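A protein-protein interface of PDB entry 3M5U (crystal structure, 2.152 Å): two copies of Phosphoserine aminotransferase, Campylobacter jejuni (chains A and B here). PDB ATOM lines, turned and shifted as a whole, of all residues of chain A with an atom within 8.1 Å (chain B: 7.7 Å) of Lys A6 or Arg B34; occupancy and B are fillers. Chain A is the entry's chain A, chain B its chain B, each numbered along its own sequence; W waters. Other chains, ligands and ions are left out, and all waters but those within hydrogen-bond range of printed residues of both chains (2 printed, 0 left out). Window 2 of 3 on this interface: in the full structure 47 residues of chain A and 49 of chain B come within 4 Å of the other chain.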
ATOM      1  N   MET A   4     -20.023 -16.167 -19.011  1.00  0.00           N
ATOM      2  CA  MET A   4     -19.098 -15.405 -19.843  1.00  0.00           C
ATOM      3  C   MET A   4     -19.246 -15.689 -21.349  1.00  0.00           C
ATOM      4  O   MET A   4     -18.249 -15.927 -22.049  1.00  0.00           O
ATOM      5  CB  MET A   4     -17.657 -15.669 -19.396  1.00  0.00           C
ATOM      6  CG  MET A   4     -17.318 -15.074 -18.038  1.00  0.00           C
ATOM      7  SD  MET A   4     -17.918 -13.211 -17.850  1.00  0.00           S
ATOM      8  CE  MET A   4     -16.952 -12.345 -19.322  1.00  0.00           C
ATOM      9  N   ARG A   5     -20.482 -15.649 -21.848  1.00  0.00           N
ATOM     10  CA  ARG A   5     -20.736 -15.928 -23.259  1.00  0.00           C
ATOM     11  C   ARG A   5     -20.026 -14.958 -24.225  1.00  0.00           C
ATOM     12  O   ARG A   5     -20.008 -13.744 -24.017  1.00  0.00           O
ATOM     13  CB  ARG A   5     -22.244 -16.006 -23.547  1.00  0.00           C
ATOM     14  CG  ARG A   5     -22.702 -17.459 -23.784  1.00  0.00           C
ATOM     15  CD  ARG A   5     -24.232 -17.663 -23.675  1.00  0.00           C
ATOM     16  NE  ARG A   5     -24.944 -17.067 -24.799  1.00  0.00           N
ATOM     17  CZ  ARG A   5     -25.043 -17.630 -25.991  1.00  0.00           C
ATOM     18  NH1 ARG A   5     -25.711 -17.028 -26.968  1.00  0.00           N
ATOM     19  NH2 ARG A   5     -24.477 -18.798 -26.207  1.00  0.00           N
ATOM     20  N   LYS A   6     -19.422 -15.518 -25.266  1.00  0.00           N
ATOM     21  CA  LYS A   6     -18.784 -14.738 -26.322  1.00  0.00           C
ATOM     22  C   LYS A   6     -19.789 -13.869 -27.084  1.00  0.00           C
ATOM     23  O   LYS A   6     -20.982 -14.182 -27.160  1.00  0.00           O
ATOM     24  CB  LYS A   6     -18.082 -15.683 -27.304  1.00  0.00           C
ATOM     25  CG  LYS A   6     -16.611 -15.984 -26.985  1.00  0.00           C
ATOM     26  CD  LYS A   6     -16.418 -16.442 -25.559  1.00  0.00           C
ATOM     27  CE  LYS A   6     -15.021 -16.990 -25.335  1.00  0.00           C
ATOM     28  NZ  LYS A   6     -14.237 -16.122 -24.392  1.00  0.00           N
ATOM     29  N   ILE A   7     -19.316 -12.766 -27.654  1.00  0.00           N
ATOM     30  CA  ILE A   7     -20.161 -12.039 -28.583  1.00  0.00           C
ATOM     31  C   ILE A   7     -19.966 -12.738 -29.900  1.00  0.00           C
ATOM     32  O   ILE A   7     -18.842 -12.863 -30.397  1.00  0.00           O
ATOM     33  CB  ILE A   7     -19.779 -10.580 -28.771  1.00  0.00           C
ATOM     34  CG1 ILE A   7     -19.844  -9.811 -27.446  1.00  0.00           C
ATOM     35  CG2 ILE A   7     -20.712  -9.905 -29.828  1.00  0.00           C
ATOM     36  CD1 ILE A   7     -19.289  -8.400 -27.585  1.00  0.00           C
ATOM     37  N   ASN A   8     -21.063 -13.186 -30.488  1.00  0.00           N
ATOM     38  CA  ASN A   8     -20.921 -14.084 -31.605  1.00  0.00           C
ATOM     39  C   ASN A   8     -21.457 -13.527 -32.900  1.00  0.00           C
ATOM     40  O   ASN A   8     -22.672 -13.393 -33.055  1.00  0.00           O
ATOM     41  CB  ASN A   8     -21.611 -15.402 -31.251  1.00  0.00           C
ATOM     42  CG  ASN A   8     -21.531 -16.433 -32.364  1.00  0.00           C
ATOM     43  OD1 ASN A   8     -20.868 -16.227 -33.403  1.00  0.00           O
ATOM     44  ND2 ASN A   8     -22.224 -17.558 -32.150  1.00  0.00           N
ATOM     45  N   PHE A   9     -20.555 -13.239 -33.844  1.00  0.00           N
ATOM     46  CA  PHE A   9     -20.935 -12.667 -35.138  1.00  0.00           C
ATOM     47  C   PHE A   9     -21.061 -13.670 -36.289  1.00  0.00           C
ATOM     48  O   PHE A   9     -21.079 -13.254 -37.455  1.00  0.00           O
ATOM     49  CB  PHE A   9     -20.018 -11.513 -35.566  1.00  0.00           C
ATOM     50  CG  PHE A   9     -19.979 -10.352 -34.607  1.00  0.00           C
ATOM     51  CD1 PHE A   9     -20.908  -9.321 -34.692  1.00  0.00           C
ATOM     52  CD2 PHE A   9     -18.982 -10.270 -33.644  1.00  0.00           C
ATOM     53  CE1 PHE A   9     -20.866  -8.231 -33.806  1.00  0.00           C
ATOM     54  CE2 PHE A   9     -18.918  -9.186 -32.758  1.00  0.00           C
ATOM     55  CZ  PHE A   9     -19.856  -8.155 -32.854  1.00  0.00           C
ATOM     56  N   THR A  15     -25.927 -16.681 -33.632  1.00  0.00           N
ATOM     57  CA  THR A  15     -26.186 -16.593 -32.210  1.00  0.00           C
ATOM     58  C   THR A  15     -27.710 -16.529 -31.932  1.00  0.00           C
ATOM     59  O   THR A  15     -28.471 -15.998 -32.732  1.00  0.00           O
ATOM     60  CB  THR A  15     -25.426 -15.391 -31.629  1.00  0.00           C
ATOM     61  OG1 THR A  15     -25.339 -15.495 -30.204  1.00  0.00           O
ATOM     62  CG2 THR A  15     -26.110 -14.020 -32.038  1.00  0.00           C
ATOM     63  N   ALA A 316      -9.679 -10.094 -31.972  1.00  0.00           N
ATOM     64  CA  ALA A 316     -11.120 -10.094 -31.706  1.00  0.00           C
ATOM     65  C   ALA A 316     -11.513 -11.296 -30.839  1.00  0.00           C
ATOM     66  O   ALA A 316     -12.249 -11.170 -29.852  1.00  0.00           O
ATOM     67  CB  ALA A 316     -11.940 -10.096 -33.027  1.00  0.00           C
ATOM     68  N   GLU A 317     -11.016 -12.458 -31.214  1.00  0.00           N
ATOM     69  CA  GLU A 317     -11.306 -13.692 -30.484  1.00  0.00           C
ATOM     70  C   GLU A 317     -10.772 -13.589 -29.058  1.00  0.00           C
ATOM     71  O   GLU A 317     -11.443 -13.938 -28.094  1.00  0.00           O
ATOM     72  CB  GLU A 317     -10.623 -14.854 -31.183  1.00  0.00           C
ATOM     73  CG  GLU A 317     -11.520 -16.014 -31.535  1.00  0.00           C
ATOM     74  CD  GLU A 317     -10.957 -16.847 -32.696  1.00  0.00           C
ATOM     75  OE1 GLU A 317      -9.751 -17.185 -32.670  1.00  0.00           O
ATOM     76  OE2 GLU A 317     -11.719 -17.154 -33.639  1.00  0.00           O
ATOM     77  N   GLU A 318      -9.549 -13.103 -28.923  1.00  0.00           N
ATOM     78  CA  GLU A 318      -8.934 -13.040 -27.611  1.00  0.00           C
ATOM     79  C   GLU A 318      -9.715 -12.086 -26.760  1.00  0.00           C
ATOM     80  O   GLU A 318      -9.680 -12.162 -25.535  1.00  0.00           O
ATOM     81  CB  GLU A 318      -7.496 -12.573 -27.706  1.00  0.00           C
ATOM     82  CG  GLU A 318      -6.565 -13.603 -28.279  1.00  0.00           C
ATOM     83  CD  GLU A 318      -5.116 -13.171 -28.139  1.00  0.00           C
ATOM     84  OE1 GLU A 318      -4.801 -12.003 -28.478  1.00  0.00           O
ATOM     85  OE2 GLU A 318      -4.301 -13.998 -27.676  1.00  0.00           O
ATOM     86  N   ALA A 319     -10.415 -11.169 -27.417  1.00  0.00           N
ATOM     87  CA  ALA A 319     -11.246 -10.231 -26.703  1.00  0.00           C
ATOM     88  C   ALA A 319     -12.737 -10.670 -26.654  1.00  0.00           C
ATOM     89  O   ALA A 319     -13.610  -9.846 -26.420  1.00  0.00           O
ATOM     90  CB  ALA A 319     -11.082  -8.817 -27.293  1.00  0.00           C
ATOM     91  N   GLY A 320     -13.007 -11.961 -26.869  1.00  0.00           N
ATOM     92  CA  GLY A 320     -14.346 -12.519 -26.703  1.00  0.00           C
ATOM     93  C   GLY A 320     -15.343 -12.267 -27.824  1.00  0.00           C
ATOM     94  O   GLY A 320     -16.573 -12.305 -27.621  1.00  0.00           O
ATOM     95  N   MET A 321     -14.838 -12.000 -29.019  1.00  0.00           N
ATOM     96  CA  MET A 321     -15.732 -11.757 -30.147  1.00  0.00           C
ATOM     97  C   MET A 321     -15.362 -12.753 -31.207  1.00  0.00           C
ATOM     98  O   MET A 321     -14.204 -12.812 -31.597  1.00  0.00           O
ATOM     99  CB  MET A 321     -15.545 -10.343 -30.703  1.00  0.00           C
ATOM    100  CG  MET A 321     -16.195  -9.264 -29.886  1.00  0.00           C
ATOM    101  SD  MET A 321     -15.672  -7.492 -30.504  1.00  0.00           S
ATOM    102  CE  MET A 321     -13.821  -7.518 -29.833  1.00  0.00           C
ATOM    103  N   ILE A 322     -16.322 -13.556 -31.652  1.00  0.00           N
ATOM    104  CA  ILE A 322     -16.020 -14.642 -32.586  1.00  0.00           C
ATOM    105  C   ILE A 322     -16.850 -14.558 -33.867  1.00  0.00           C
ATOM    106  O   ILE A 322     -17.848 -13.842 -33.930  1.00  0.00           O
ATOM    107  CB  ILE A 322     -16.244 -16.045 -31.933  1.00  0.00           C
ATOM    108  CG1 ILE A 322     -17.735 -16.333 -31.740  1.00  0.00           C
ATOM    109  CG2 ILE A 322     -15.510 -16.153 -30.590  1.00  0.00           C
ATOM    110  CD1 ILE A 322     -18.026 -17.803 -31.273  1.00  0.00           C
ATOM    111  N   GLY A 323     -16.451 -15.311 -34.878  1.00  0.00           N
ATOM    112  CA  GLY A 323     -17.278 -15.459 -36.057  1.00  0.00           C
ATOM    113  C   GLY A 323     -17.038 -14.404 -37.108  1.00  0.00           C
ATOM    114  O   GLY A 323     -17.817 -14.283 -38.043  1.00  0.00           O
ATOM    115  N   LEU A 341     -28.218  -9.939 -32.103  1.00  0.00           N
ATOM    116  CA  LEU A 341     -27.100  -9.082 -31.697  1.00  0.00           C
ATOM    117  C   LEU A 341     -27.631  -7.704 -31.346  1.00  0.00           C
ATOM    118  O   LEU A 341     -28.536  -7.183 -32.021  1.00  0.00           O
ATOM    119  CB  LEU A 341     -26.030  -9.005 -32.785  1.00  0.00           C
ATOM    120  CG  LEU A 341     -25.104 -10.200 -32.642  1.00  0.00           C
ATOM    121  CD1 LEU A 341     -24.247 -10.339 -33.859  1.00  0.00           C
ATOM    122  CD2 LEU A 341     -24.254 -10.021 -31.398  1.00  0.00           C
ATOM    123  N   GLN A 345     -23.351  -4.738 -28.234  1.00  0.00           N
ATOM    124  CA  GLN A 345     -22.342  -5.688 -28.703  1.00  0.00           C
ATOM    125  C   GLN A 345     -21.586  -5.144 -29.944  1.00  0.00           C
ATOM    126  O   GLN A 345     -20.369  -5.360 -30.111  1.00  0.00           O
ATOM    127  CB  GLN A 345     -22.976  -7.055 -28.963  1.00  0.00           C
ATOM    128  CG  GLN A 345     -23.456  -7.722 -27.680  1.00  0.00           C
ATOM    129  CD  GLN A 345     -24.376  -8.907 -27.943  1.00  0.00           C
ATOM    130  OE1 GLN A 345     -25.321  -8.806 -28.720  1.00  0.00           O
ATOM    131  NE2 GLN A 345     -24.097 -10.033 -27.301  1.00  0.00           N
ATOM    132  N   CYS B  29     -26.012 -23.606 -23.254  1.00  0.00           N
ATOM    133  CA  CYS B  29     -25.669 -22.196 -23.429  1.00  0.00           C
ATOM    134  C   CYS B  29     -24.169 -22.024 -23.594  1.00  0.00           C
ATOM    135  O   CYS B  29     -23.678 -20.960 -23.979  1.00  0.00           O
ATOM    136  CB  CYS B  29     -26.150 -21.370 -22.217  1.00  0.00           C
ATOM    137  SG  CYS B  29     -27.970 -21.377 -21.958  1.00  0.00           S
ATOM    138  N   ASP B  30     -23.432 -23.079 -23.290  1.00  0.00           N
ATOM    139  CA  ASP B  30     -21.991 -22.961 -23.115  1.00  0.00           C
ATOM    140  C   ASP B  30     -21.355 -24.328 -23.307  1.00  0.00           C
ATOM    141  O   ASP B  30     -21.030 -25.035 -22.352  1.00  0.00           O
ATOM    142  CB  ASP B  30     -21.684 -22.442 -21.718  1.00  0.00           C
ATOM    143  CG  ASP B  30     -20.232 -22.035 -21.560  1.00  0.00           C
ATOM    144  OD1 ASP B  30     -19.534 -21.930 -22.590  1.00  0.00           O
ATOM    145  OD2 ASP B  30     -19.796 -21.817 -20.408  1.00  0.00           O
ATOM    146  N   TYR B  31     -21.212 -24.696 -24.569  1.00  0.00           N
ATOM    147  CA  TYR B  31     -20.659 -25.971 -24.949  1.00  0.00           C
ATOM    148  C   TYR B  31     -19.207 -26.093 -24.483  1.00  0.00           C
ATOM    149  O   TYR B  31     -18.363 -25.277 -24.852  1.00  0.00           O
ATOM    150  CB  TYR B  31     -20.751 -26.086 -26.460  1.00  0.00           C
ATOM    151  CG  TYR B  31     -20.114 -27.321 -27.036  1.00  0.00           C
ATOM    152  CD1 TYR B  31     -20.693 -28.580 -26.853  1.00  0.00           C
ATOM    153  CD2 TYR B  31     -18.955 -27.230 -27.789  1.00  0.00           C
ATOM    154  CE1 TYR B  31     -20.115 -29.723 -27.399  1.00  0.00           C
ATOM    155  CE2 TYR B  31     -18.374 -28.348 -28.328  1.00  0.00           C
ATOM    156  CZ  TYR B  31     -18.955 -29.595 -28.137  1.00  0.00           C
ATOM    157  OH  TYR B  31     -18.361 -30.705 -28.690  1.00  0.00           O
ATOM    158  N   GLN B  32     -18.921 -27.109 -23.672  1.00  0.00           N
ATOM    159  CA  GLN B  32     -17.552 -27.361 -23.217  1.00  0.00           C
ATOM    160  C   GLN B  32     -16.871 -26.100 -22.674  1.00  0.00           C
ATOM    161  O   GLN B  32     -15.648 -25.915 -22.816  1.00  0.00           O
ATOM    162  CB  GLN B  32     -16.712 -27.975 -24.349  1.00  0.00           C
ATOM    163  CG  GLN B  32     -17.307 -29.272 -24.900  1.00  0.00           C
ATOM    164  CD  GLN B  32     -16.468 -29.905 -25.994  1.00  0.00           C
ATOM    165  OE1 GLN B  32     -15.660 -29.238 -26.650  1.00  0.00           O
ATOM    166  NE2 GLN B  32     -16.673 -31.192 -26.212  1.00  0.00           N
ATOM    167  N   GLY B  33     -17.665 -25.225 -22.062  1.00  0.00           N
ATOM    168  CA  GLY B  33     -17.133 -23.979 -21.526  1.00  0.00           C
ATOM    169  C   GLY B  33     -16.551 -23.025 -22.561  1.00  0.00           C
ATOM    170  O   GLY B  33     -15.865 -22.057 -22.208  1.00  0.00           O
ATOM    171  N   ARG B  34     -16.840 -23.261 -23.842  1.00  0.00           N
ATOM    172  CA  ARG B  34     -16.309 -22.392 -24.903  1.00  0.00           C
ATOM    173  C   ARG B  34     -17.034 -21.035 -25.137  1.00  0.00           C
ATOM    174  O   ARG B  34     -16.587 -20.246 -25.968  1.00  0.00           O
ATOM    175  CB  ARG B  34     -16.237 -23.154 -26.232  1.00  0.00           C
ATOM    176  CG  ARG B  34     -15.465 -24.451 -26.175  1.00  0.00           C
ATOM    177  CD  ARG B  34     -15.692 -25.264 -27.464  1.00  0.00           C
ATOM    178  NE  ARG B  34     -14.993 -26.545 -27.430  1.00  0.00           N
ATOM    179  CZ  ARG B  34     -13.692 -26.705 -27.680  1.00  0.00           C
ATOM    180  NH1 ARG B  34     -12.928 -25.663 -28.000  1.00  0.00           N
ATOM    181  NH2 ARG B  34     -13.152 -27.915 -27.611  1.00  0.00           N
ATOM    182  N   GLY B  35     -18.150 -20.766 -24.457  1.00  0.00           N
ATOM    183  CA  GLY B  35     -18.795 -19.456 -24.560  1.00  0.00           C
ATOM    184  C   GLY B  35     -19.899 -19.313 -25.618  1.00  0.00           C
ATOM    185  O   GLY B  35     -20.254 -18.191 -26.028  1.00  0.00           O
ATOM    186  N   TYR B  36     -20.432 -20.450 -26.062  1.00  0.00           N
ATOM    187  CA  TYR B  36     -21.543 -20.487 -27.015  1.00  0.00           C
ATOM    188  C   TYR B  36     -22.175 -21.868 -27.021  1.00  0.00           C
ATOM    189  O   TYR B  36     -21.611 -22.837 -26.515  1.00  0.00           O
ATOM    190  CB  TYR B  36     -21.085 -20.162 -28.442  1.00  0.00           C
ATOM    191  CG  TYR B  36     -19.925 -21.037 -28.912  1.00  0.00           C
ATOM    192  CD1 TYR B  36     -20.143 -22.282 -29.534  1.00  0.00           C
ATOM    193  CD2 TYR B  36     -18.611 -20.622 -28.721  1.00  0.00           C
ATOM    194  CE1 TYR B  36     -19.066 -23.082 -29.946  1.00  0.00           C
ATOM    195  CE2 TYR B  36     -17.546 -21.403 -29.127  1.00  0.00           C
ATOM    196  CZ  TYR B  36     -17.773 -22.624 -29.737  1.00  0.00           C
ATOM    197  OH  TYR B  36     -16.689 -23.352 -30.152  1.00  0.00           O
ATOM    198  N   SER B  37     -23.349 -21.957 -27.611  1.00  0.00           N
ATOM    199  CA  SER B  37     -24.102 -23.208 -27.616  1.00  0.00           C
ATOM    200  C   SER B  37     -23.652 -24.046 -28.789  1.00  0.00           C
ATOM    201  O   SER B  37     -23.276 -23.535 -29.844  1.00  0.00           O
ATOM    202  CB  SER B  37     -25.615 -22.954 -27.769  1.00  0.00           C
ATOM    203  OG  SER B  37     -26.309 -24.172 -27.990  1.00  0.00           O
ATOM    204  N   GLU B  40     -25.111 -23.010 -32.000  1.00  0.00           N
ATOM    205  CA  GLU B  40     -24.906 -21.611 -32.388  1.00  0.00           C
ATOM    206  C   GLU B  40     -23.652 -21.312 -33.219  1.00  0.00           C
ATOM    207  O   GLU B  40     -23.368 -20.125 -33.563  1.00  0.00           O
ATOM    208  CB  GLU B  40     -24.814 -20.769 -31.146  1.00  0.00           C
ATOM    209  CG  GLU B  40     -26.084 -20.308 -30.617  1.00  0.00           C
ATOM    210  CD  GLU B  40     -25.835 -19.548 -29.372  1.00  0.00           C
ATOM    211  OE1 GLU B  40     -24.791 -19.842 -28.730  1.00  0.00           O
ATOM    212  OE2 GLU B  40     -26.647 -18.653 -29.043  1.00  0.00           O
ATOM    213  N   ILE B  41     -22.871 -22.349 -33.512  1.00  0.00           N
ATOM    214  CA  ILE B  41     -21.701 -22.099 -34.337  1.00  0.00           C
ATOM    215  C   ILE B  41     -21.716 -22.812 -35.677  1.00  0.00           C
ATOM    216  O   ILE B  41     -22.509 -23.733 -35.913  1.00  0.00           O
ATOM    217  CB  ILE B  41     -20.390 -22.425 -33.616  1.00  0.00           C
ATOM    218  CG1 ILE B  41     -20.434 -23.861 -33.051  1.00  0.00           C
ATOM    219  CG2 ILE B  41     -20.081 -21.335 -32.592  1.00  0.00           C
ATOM    220  CD1 ILE B  41     -19.055 -24.452 -32.814  1.00  0.00           C
ATOM    221  N   LYS B  46     -13.559 -26.339 -36.438  1.00  0.00           N
ATOM    222  CA  LYS B  46     -12.955 -27.595 -36.018  1.00  0.00           C
ATOM    223  C   LYS B  46     -13.767 -28.186 -34.886  1.00  0.00           C
ATOM    224  O   LYS B  46     -13.716 -29.380 -34.616  1.00  0.00           O
ATOM    225  CB  LYS B  46     -11.497 -27.381 -35.596  1.00  0.00           C
ATOM    226  CG  LYS B  46     -10.517 -27.449 -36.781  1.00  0.00           C
ATOM    227  CD  LYS B  46      -9.529 -26.269 -36.838  1.00  0.00           C
ATOM    228  CE  LYS B  46      -8.599 -26.382 -38.067  1.00  0.00           C
ATOM    229  NZ  LYS B  46      -7.137 -26.143 -37.769  1.00  0.00           N
ATOM    230  N   VAL B  47     -14.522 -27.333 -34.213  1.00  0.00           N
ATOM    231  CA  VAL B  47     -15.323 -27.797 -33.085  1.00  0.00           C
ATOM    232  C   VAL B  47     -16.544 -28.622 -33.568  1.00  0.00           C
ATOM    233  O   VAL B  47     -16.763 -29.731 -33.101  1.00  0.00           O
ATOM    234  CB  VAL B  47     -15.715 -26.621 -32.165  1.00  0.00           C
ATOM    235  CG1 VAL B  47     -16.396 -27.118 -30.927  1.00  0.00           C
ATOM    236  CG2 VAL B  47     -14.457 -25.793 -31.792  1.00  0.00           C
ATOM    237  N   PHE B  48     -17.300 -28.111 -34.533  1.00  0.00           N
ATOM    238  CA  PHE B  48     -18.389 -28.904 -35.094  1.00  0.00           C
ATOM    239  C   PHE B  48     -17.881 -30.096 -35.850  1.00  0.00           C
ATOM    240  O   PHE B  48     -18.518 -31.129 -35.847  1.00  0.00           O
ATOM    241  CB  PHE B  48     -19.342 -28.125 -36.015  1.00  0.00           C
ATOM    242  CG  PHE B  48     -20.472 -28.993 -36.553  1.00  0.00           C
ATOM    243  CD1 PHE B  48     -21.586 -29.284 -35.758  1.00  0.00           C
ATOM    244  CD2 PHE B  48     -20.390 -29.576 -37.816  1.00  0.00           C
ATOM    245  CE1 PHE B  48     -22.612 -30.112 -36.233  1.00  0.00           C
ATOM    246  CE2 PHE B  48     -21.430 -30.407 -38.298  1.00  0.00           C
ATOM    247  CZ  PHE B  48     -22.524 -30.672 -37.500  1.00  0.00           C
ATOM    248  N   GLU B  50     -15.340 -31.992 -35.283  1.00  0.00           N
ATOM    249  CA  GLU B  50     -14.990 -33.084 -34.374  1.00  0.00           C
ATOM    250  C   GLU B  50     -16.204 -33.954 -33.978  1.00  0.00           C
ATOM    251  O   GLU B  50     -16.141 -35.187 -33.936  1.00  0.00           O
ATOM    252  CB  GLU B  50     -14.393 -32.492 -33.114  1.00  0.00           C
ATOM    253  CG  GLU B  50     -13.416 -33.392 -32.427  1.00  0.00           C
ATOM    254  CD  GLU B  50     -12.813 -32.709 -31.234  1.00  0.00           C
ATOM    255  OE1 GLU B  50     -13.531 -32.593 -30.212  1.00  0.00           O
ATOM    256  OE2 GLU B  50     -11.639 -32.269 -31.335  1.00  0.00           O
HETATM  257  O   HOH W   1     -23.603 -17.535 -29.745  1.00  0.00           O
HETATM  258  O   HOH W   2     -21.718 -16.991 -27.771  1.00  0.00           O
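Arg B34 touches just one residue of chain A: Lys A6 (3.7 Å).
Printed residues of chain A within 4 Å of Tyr B36: Arg A5 and Ile A322.
Printed residues of chain B within 4 Å of Ile A322: Tyr B36.
Phe A9 touches none of the printed residues of chain B.
Leu A341 touches none of the printed residues of chain B.
The nearest printed residue of chain B that does not touch Arg A5 is Asp B30 (5.3 Å).
Hydrophobic or aromatic side chains of chain A within 4 Å of the printed part of chain B: Ile A322.
Hydrophobic or aromatic side chains of chain B within 4 Å of the printed part of chain A: Tyr B36.
Among the printed residues, 10 pairs touch across the chains.
Gly B35 touches Arg A5 (O to CG, 3.4 Å).
Tyr B36 touches Arg A5.
NH2 of Arg A5 touches N of Ser B37, 3.6 Å away.
Arg B34 touches Lys A6 (O to CE, 3.7 Å).
Glu B40 touches Thr A15 (OE2 to OG1, 3.6 Å).
Tyr B36 touches Ile A322 (CD2 to CD1, 3.8 Å).
The backbone carbonyl oxygen of Ile A7 sits at hydrogen-bond distance from the backbone NH of Ile A322 (2.9 Å).
N of Phe A9 is in hydrogen-bond range of O of Ile A322, at 2.8 Å.
N of Arg B34 is in hydrogen-bond range of OD1 of Asp B30 (3.3 Å).
N of Tyr B31 sits at hydrogen-bond distance from O of Tyr B36.
The side-chain amide oxygen of Gln B32 is in hydrogen-bond range of the guanidinium group of Arg B34, at 2.9 Å.
The backbone NH of Ser B37 is in hydrogen-bond range of the side-chain carboxylate of Glu B40, 2.8 Å away.
The backbone carbonyl oxygen of Cys B29 is in hydrogen-bond range of the guanidinium group of Arg A5, at 3.2 Å.
The side-chain carboxylate of Glu B40 is in salt-bridge range of the guanidinium group of Arg A5 (2.7 Å).
The backbone NH (N) of Lys A6 lies within hydrogen-bond range of the backbone carbonyl oxygen (O) of Gly B35.
ND2 of Asn A8 lies within hydrogen-bond range of O of Glu B40, at 3.1 Å.
Water W2 bridges O of Gly B35 (2.6 Å) and O of Lys A6 (3.0 Å).
Water W1 lies within hydrogen-bond range of the side-chain hydroxyl of Thr A15 (2.7 Å), the side-chain amide nitrogen of Asn A8 (2.8 Å) and the side-chain carboxylate of Glu B40 (2.8 Å).
No position is printed for both chains.
Of the 10 pairs that touch across the chains among the printed residues, none has its exchanged pair printed and touching as well.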
